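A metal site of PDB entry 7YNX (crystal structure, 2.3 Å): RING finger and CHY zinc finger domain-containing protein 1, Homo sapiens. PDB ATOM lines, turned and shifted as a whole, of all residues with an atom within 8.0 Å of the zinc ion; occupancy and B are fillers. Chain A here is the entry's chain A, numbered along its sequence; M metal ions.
The backbone NH (N) of Cys 120 sits at hydrogen-bond distance from the backbone carbonyl oxygen (O) of Leu 125 (2.9 Å). SG of Cys 123 sits close to N of Ile 138 (3.6 Å). The backbone carbonyl oxygen of Leu 131 is in hydrogen-bond range of a ring nitrogen (ND1) of His 135 (2.6 Å). The side-chain sulfur of Cys 120 sits close to the backbone NH of Lys 122 (3.6 Å).
The zinc ion is bound by NE2 of His 135, at 2.2 Å. SG of Cys 137 is bound to the zinc ion, at 2.4 Å. SG of Cys 123 binds the zinc ion (2.4 Å). The zinc ion is bound by the side-chain sulfur (SG) of Cys 120, at 2.5 Å.
Of the 21 residues printed, 4 come within 4 Å of the zinc ion. The nearest printed residue that does not touch the zinc ion is Lys 122 (4.5 Å).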
ATOM      1  N   PHE A 118       9.558  -2.767 -21.321  1.00  0.00           N
ATOM      2  CA  PHE A 118      10.667  -2.329 -22.145  1.00  0.00           C
ATOM      3  C   PHE A 118      10.520  -0.827 -22.358  1.00  0.00           C
ATOM      4  O   PHE A 118       9.400  -0.305 -22.385  1.00  0.00           O
ATOM      5  CB  PHE A 118      10.698  -3.050 -23.511  1.00  0.00           C
ATOM      6  CG  PHE A 118       9.723  -2.482 -24.514  1.00  0.00           C
ATOM      7  CD1 PHE A 118       8.384  -2.835 -24.467  1.00  0.00           C
ATOM      8  CD2 PHE A 118      10.139  -1.575 -25.471  1.00  0.00           C
ATOM      9  CE1 PHE A 118       7.469  -2.307 -25.384  1.00  0.00           C
ATOM     10  CE2 PHE A 118       9.240  -1.041 -26.391  1.00  0.00           C
ATOM     11  CZ  PHE A 118       7.908  -1.398 -26.350  1.00  0.00           C
ATOM     12  N   HIS A 119      11.636  -0.136 -22.492  1.00  0.00           N
ATOM     13  CA  HIS A 119      11.575   1.286 -22.786  1.00  0.00           C
ATOM     14  C   HIS A 119      11.501   1.473 -24.297  1.00  0.00           C
ATOM     15  O   HIS A 119      12.357   0.982 -25.036  1.00  0.00           O
ATOM     16  CB  HIS A 119      12.781   2.033 -22.211  1.00  0.00           C
ATOM     17  CG  HIS A 119      12.618   3.519 -22.261  1.00  0.00           C
ATOM     18  ND1 HIS A 119      12.114   4.256 -21.216  1.00  0.00           N
ATOM     19  CD2 HIS A 119      12.827   4.402 -23.276  1.00  0.00           C
ATOM     20  CE1 HIS A 119      12.041   5.523 -21.556  1.00  0.00           C
ATOM     21  NE2 HIS A 119      12.474   5.644 -22.806  1.00  0.00           N
ATOM     22  N   CYS A 120      10.464   2.165 -24.756  1.00  0.00           N
ATOM     23  CA  CYS A 120      10.385   2.530 -26.162  1.00  0.00           C
ATOM     24  C   CYS A 120      11.124   3.842 -26.365  1.00  0.00           C
ATOM     25  O   CYS A 120      10.744   4.861 -25.775  1.00  0.00           O
ATOM     26  CB  CYS A 120       8.937   2.670 -26.623  1.00  0.00           C
ATOM     27  SG  CYS A 120       8.843   3.275 -28.323  1.00  0.00           S
ATOM     28  N   LEU A 121      12.188   3.808 -27.173  1.00  0.00           N
ATOM     29  CA  LEU A 121      12.963   5.021 -27.420  1.00  0.00           C
ATOM     30  C   LEU A 121      12.086   6.137 -27.981  1.00  0.00           C
ATOM     31  O   LEU A 121      12.123   7.278 -27.501  1.00  0.00           O
ATOM     32  CB  LEU A 121      14.112   4.731 -28.379  1.00  0.00           C
ATOM     33  CG  LEU A 121      15.104   3.605 -28.050  1.00  0.00           C
ATOM     34  CD1 LEU A 121      15.953   3.266 -29.271  1.00  0.00           C
ATOM     35  CD2 LEU A 121      15.995   3.957 -26.856  1.00  0.00           C
ATOM     36  N   LYS A 122      11.278   5.828 -28.992  1.00  0.00           N
ATOM     37  CA  LYS A 122      10.517   6.867 -29.666  1.00  0.00           C
ATOM     38  C   LYS A 122       9.487   7.505 -28.745  1.00  0.00           C
ATOM     39  O   LYS A 122       9.513   8.723 -28.491  1.00  0.00           O
ATOM     40  CB  LYS A 122       9.836   6.311 -30.929  1.00  0.00           C
ATOM     41  CG  LYS A 122       9.155   7.390 -31.777  1.00  0.00           C
ATOM     42  CD  LYS A 122       8.993   6.980 -33.230  1.00  0.00           C
ATOM     43  CE  LYS A 122       9.855   7.812 -34.152  1.00  0.00           C
ATOM     44  NZ  LYS A 122       9.655   7.430 -35.582  1.00  0.00           N
ATOM     45  N   CYS A 123       8.544   6.705 -28.233  1.00  0.00           N
ATOM     46  CA  CYS A 123       7.539   7.293 -27.348  1.00  0.00           C
ATOM     47  C   CYS A 123       8.177   7.817 -26.080  1.00  0.00           C
ATOM     48  O   CYS A 123       7.642   8.735 -25.450  1.00  0.00           O
ATOM     49  CB  CYS A 123       6.459   6.279 -27.020  1.00  0.00           C
ATOM     50  SG  CYS A 123       5.544   5.725 -28.475  1.00  0.00           S
ATOM     51  N   ASN A 124       9.320   7.226 -25.696  1.00  0.00           N
ATOM     52  CA  ASN A 124      10.182   7.658 -24.608  1.00  0.00           C
ATOM     53  C   ASN A 124       9.572   7.384 -23.233  1.00  0.00           C
ATOM     54  O   ASN A 124       9.732   8.177 -22.316  1.00  0.00           O
ATOM     55  CB  ASN A 124      10.576   9.121 -24.741  1.00  0.00           C
ATOM     56  CG  ASN A 124      12.016   9.344 -24.362  1.00  0.00           C
ATOM     57  OD1 ASN A 124      12.667   8.431 -23.873  1.00  0.00           O
ATOM     58  ND2 ASN A 124      12.530  10.559 -24.598  1.00  0.00           N
ATOM     59  N   LEU A 125       8.917   6.237 -23.088  1.00  0.00           N
ATOM     60  CA  LEU A 125       8.546   5.736 -21.767  1.00  0.00           C
ATOM     61  C   LEU A 125       8.645   4.213 -21.777  1.00  0.00           C
ATOM     62  O   LEU A 125       8.853   3.583 -22.815  1.00  0.00           O
ATOM     63  CB  LEU A 125       7.145   6.177 -21.339  1.00  0.00           C
ATOM     64  CG  LEU A 125       5.925   5.437 -21.870  1.00  0.00           C
ATOM     65  CD1 LEU A 125       4.692   6.041 -21.227  1.00  0.00           C
ATOM     66  CD2 LEU A 125       5.832   5.510 -23.380  1.00  0.00           C
ATOM     67  N   LEU A 127       7.084   0.544 -21.538  1.00  0.00           N
ATOM     68  CA  LEU A 127       5.841  -0.060 -21.972  1.00  0.00           C
ATOM     69  C   LEU A 127       5.842  -1.550 -21.668  1.00  0.00           C
ATOM     70  O   LEU A 127       6.897  -2.195 -21.634  1.00  0.00           O
ATOM     71  CB  LEU A 127       5.608   0.157 -23.479  1.00  0.00           C
ATOM     72  CG  LEU A 127       5.310   1.606 -23.891  1.00  0.00           C
ATOM     73  CD1 LEU A 127       4.940   1.706 -25.361  1.00  0.00           C
ATOM     74  CD2 LEU A 127       4.194   2.147 -23.030  1.00  0.00           C
ATOM     75  N   LEU A 131       3.711  -4.932 -26.036  1.00  0.00           N
ATOM     76  CA  LEU A 131       3.652  -3.855 -27.022  1.00  0.00           C
ATOM     77  C   LEU A 131       4.963  -3.664 -27.789  1.00  0.00           C
ATOM     78  O   LEU A 131       5.051  -2.745 -28.624  1.00  0.00           O
ATOM     79  CB  LEU A 131       3.289  -2.530 -26.347  1.00  0.00           C
ATOM     80  CG  LEU A 131       1.912  -2.519 -25.703  1.00  0.00           C
ATOM     81  CD1 LEU A 131       1.698  -1.231 -24.934  1.00  0.00           C
ATOM     82  CD2 LEU A 131       0.798  -2.746 -26.751  1.00  0.00           C
ATOM     83  N   GLY A 133       7.486  -3.675 -30.552  1.00  0.00           N
ATOM     84  CA  GLY A 133       7.241  -3.842 -31.984  1.00  0.00           C
ATOM     85  C   GLY A 133       5.788  -4.054 -32.337  1.00  0.00           C
ATOM     86  O   GLY A 133       5.495  -4.538 -33.432  1.00  0.00           O
ATOM     87  N   ARG A 134       4.859  -3.675 -31.469  1.00  0.00           N
ATOM     88  CA  ARG A 134       3.456  -3.991 -31.647  1.00  0.00           C
ATOM     89  C   ARG A 134       2.576  -2.826 -31.174  1.00  0.00           C
ATOM     90  O   ARG A 134       1.508  -3.028 -30.585  1.00  0.00           O
ATOM     91  CB  ARG A 134       3.103  -5.285 -30.923  1.00  0.00           C
ATOM     92  CG  ARG A 134       3.110  -6.520 -31.843  1.00  0.00           C
ATOM     93  CD  ARG A 134       4.281  -7.476 -31.556  1.00  0.00           C
ATOM     94  NE  ARG A 134       4.297  -8.611 -32.494  1.00  0.00           N
ATOM     95  CZ  ARG A 134       5.239  -8.818 -33.420  1.00  0.00           C
ATOM     96  NH1 ARG A 134       6.270  -7.986 -33.552  1.00  0.00           N
ATOM     97  NH2 ARG A 134       5.164  -9.882 -34.214  1.00  0.00           N
ATOM     98  N   HIS A 135       3.009  -1.591 -31.442  1.00  0.00           N
ATOM     99  CA  HIS A 135       2.248  -0.405 -31.108  1.00  0.00           C
ATOM    100  C   HIS A 135       2.681   0.737 -32.031  1.00  0.00           C
ATOM    101  O   HIS A 135       3.755   0.679 -32.646  1.00  0.00           O
ATOM    102  CB  HIS A 135       2.429  -0.002 -29.631  1.00  0.00           C
ATOM    103  CG  HIS A 135       3.766   0.581 -29.321  1.00  0.00           C
ATOM    104  ND1 HIS A 135       4.885  -0.204 -29.111  1.00  0.00           N
ATOM    105  CD2 HIS A 135       4.174   1.859 -29.193  1.00  0.00           C
ATOM    106  CE1 HIS A 135       5.927   0.567 -28.872  1.00  0.00           C
ATOM    107  NE2 HIS A 135       5.523   1.832 -28.914  1.00  0.00           N
ATOM    108  N   LYS A 136       1.839   1.763 -32.132  1.00  0.00           N
ATOM    109  CA  LYS A 136       2.133   2.909 -32.983  1.00  0.00           C
ATOM    110  C   LYS A 136       2.867   3.973 -32.165  1.00  0.00           C
ATOM    111  O   LYS A 136       2.346   4.444 -31.151  1.00  0.00           O
ATOM    112  CB  LYS A 136       0.850   3.493 -33.583  1.00  0.00           C
ATOM    113  CG  LYS A 136       0.358   2.839 -34.904  1.00  0.00           C
ATOM    114  CD  LYS A 136       0.443   1.288 -34.911  1.00  0.00           C
ATOM    115  CE  LYS A 136      -0.709   0.623 -34.151  1.00  0.00           C
ATOM    116  NZ  LYS A 136      -0.467  -0.848 -33.968  1.00  0.00           N
ATOM    117  N   CYS A 137       4.076   4.335 -32.597  1.00  0.00           N
ATOM    118  CA  CYS A 137       4.862   5.301 -31.838  1.00  0.00           C
ATOM    119  C   CYS A 137       4.530   6.725 -32.255  1.00  0.00           C
ATOM    120  O   CYS A 137       4.420   7.018 -33.450  1.00  0.00           O
ATOM    121  CB  CYS A 137       6.367   5.092 -32.049  1.00  0.00           C
ATOM    122  SG  CYS A 137       7.143   3.534 -31.488  1.00  0.00           S
ATOM    123  N   ILE A 138       4.399   7.619 -31.278  1.00  0.00           N
ATOM    124  CA  ILE A 138       4.325   9.056 -31.502  1.00  0.00           C
ATOM    125  C   ILE A 138       5.488   9.704 -30.774  1.00  0.00           C
ATOM    126  O   ILE A 138       5.699   9.439 -29.585  1.00  0.00           O
ATOM    127  CB  ILE A 138       2.982   9.661 -31.032  1.00  0.00           C
ATOM    128  CG1 ILE A 138       1.822   8.945 -31.701  1.00  0.00           C
ATOM    129  CG2 ILE A 138       2.957  11.179 -31.300  1.00  0.00           C
ATOM    130  CD1 ILE A 138       0.455   9.327 -31.172  1.00  0.00           C
ATOM    131  N   GLU A 139       6.222  10.576 -31.479  1.00  0.00           N
ATOM    132  CA  GLU A 139       7.492  11.115 -30.996  1.00  0.00           C
ATOM    133  C   GLU A 139       7.333  11.815 -29.655  1.00  0.00           C
ATOM    134  O   GLU A 139       6.646  12.844 -29.569  1.00  0.00           O
ATOM    135  CB  GLU A 139       8.078  12.088 -32.019  1.00  0.00           C
ATOM    136  CG  GLU A 139       9.264  11.544 -32.807  1.00  0.00           C
ATOM    137  CD  GLU A 139      10.516  11.399 -31.956  1.00  0.00           C
ATOM    138  OE1 GLU A 139      10.557  12.017 -30.872  1.00  0.00           O
ATOM    139  OE2 GLU A 139      11.454  10.684 -32.371  1.00  0.00           O
ATOM    140  N   ASN A 140       7.983  11.260 -28.621  1.00  0.00           N
ATOM    141  CA  ASN A 140       7.996  11.824 -27.272  1.00  0.00           C
ATOM    142  C   ASN A 140       6.588  12.093 -26.749  1.00  0.00           C
ATOM    143  O   ASN A 140       6.369  13.044 -25.988  1.00  0.00           O
ATOM    144  CB  ASN A 140       8.829  13.111 -27.224  1.00  0.00           C
ATOM    145  CG  ASN A 140      10.319  12.835 -27.227  1.00  0.00           C
ATOM    146  OD1 ASN A 140      10.776  11.805 -26.714  1.00  0.00           O
ATOM    147  ND2 ASN A 140      11.092  13.737 -27.818  1.00  0.00           N
ATOM    148  N   VAL A 141       5.629  11.246 -27.152  1.00  0.00           N
ATOM    149  CA  VAL A 141       4.255  11.430 -26.700  1.00  0.00           C
ATOM    150  C   VAL A 141       4.171  11.317 -25.176  1.00  0.00           C
ATOM    151  O   VAL A 141       3.326  11.963 -24.548  1.00  0.00           O
ATOM    152  CB  VAL A 141       3.313  10.425 -27.394  1.00  0.00           C
ATOM    153  CG1 VAL A 141       3.628   8.992 -26.988  1.00  0.00           C
ATOM    154  CG2 VAL A 141       1.846  10.781 -27.106  1.00  0.00           C
ATOM    155  N   VAL A 162      -1.934   3.283 -23.456  1.00  0.00           N
ATOM    156  CA  VAL A 162      -1.653   3.539 -24.864  1.00  0.00           C
ATOM    157  C   VAL A 162      -2.934   3.258 -25.648  1.00  0.00           C
ATOM    158  O   VAL A 162      -3.454   2.143 -25.601  1.00  0.00           O
ATOM    159  CB  VAL A 162      -0.493   2.675 -25.366  1.00  0.00           C
ATOM    160  CG1 VAL A 162       0.010   3.181 -26.709  1.00  0.00           C
ATOM    161  CG2 VAL A 162       0.623   2.655 -24.342  1.00  0.00           C
ATOM    162  N   GLY A 166      -1.912   5.366 -30.550  1.00  0.00           N
ATOM    163  CA  GLY A 166      -0.616   5.740 -30.021  1.00  0.00           C
ATOM    164  C   GLY A 166      -0.659   6.918 -29.073  1.00  0.00           C
ATOM    165  O   GLY A 166       0.383   7.295 -28.526  1.00  0.00           O
HETATM  166 ZN    ZN M   1       6.568   3.704 -29.195  1.00  0.00          ZN
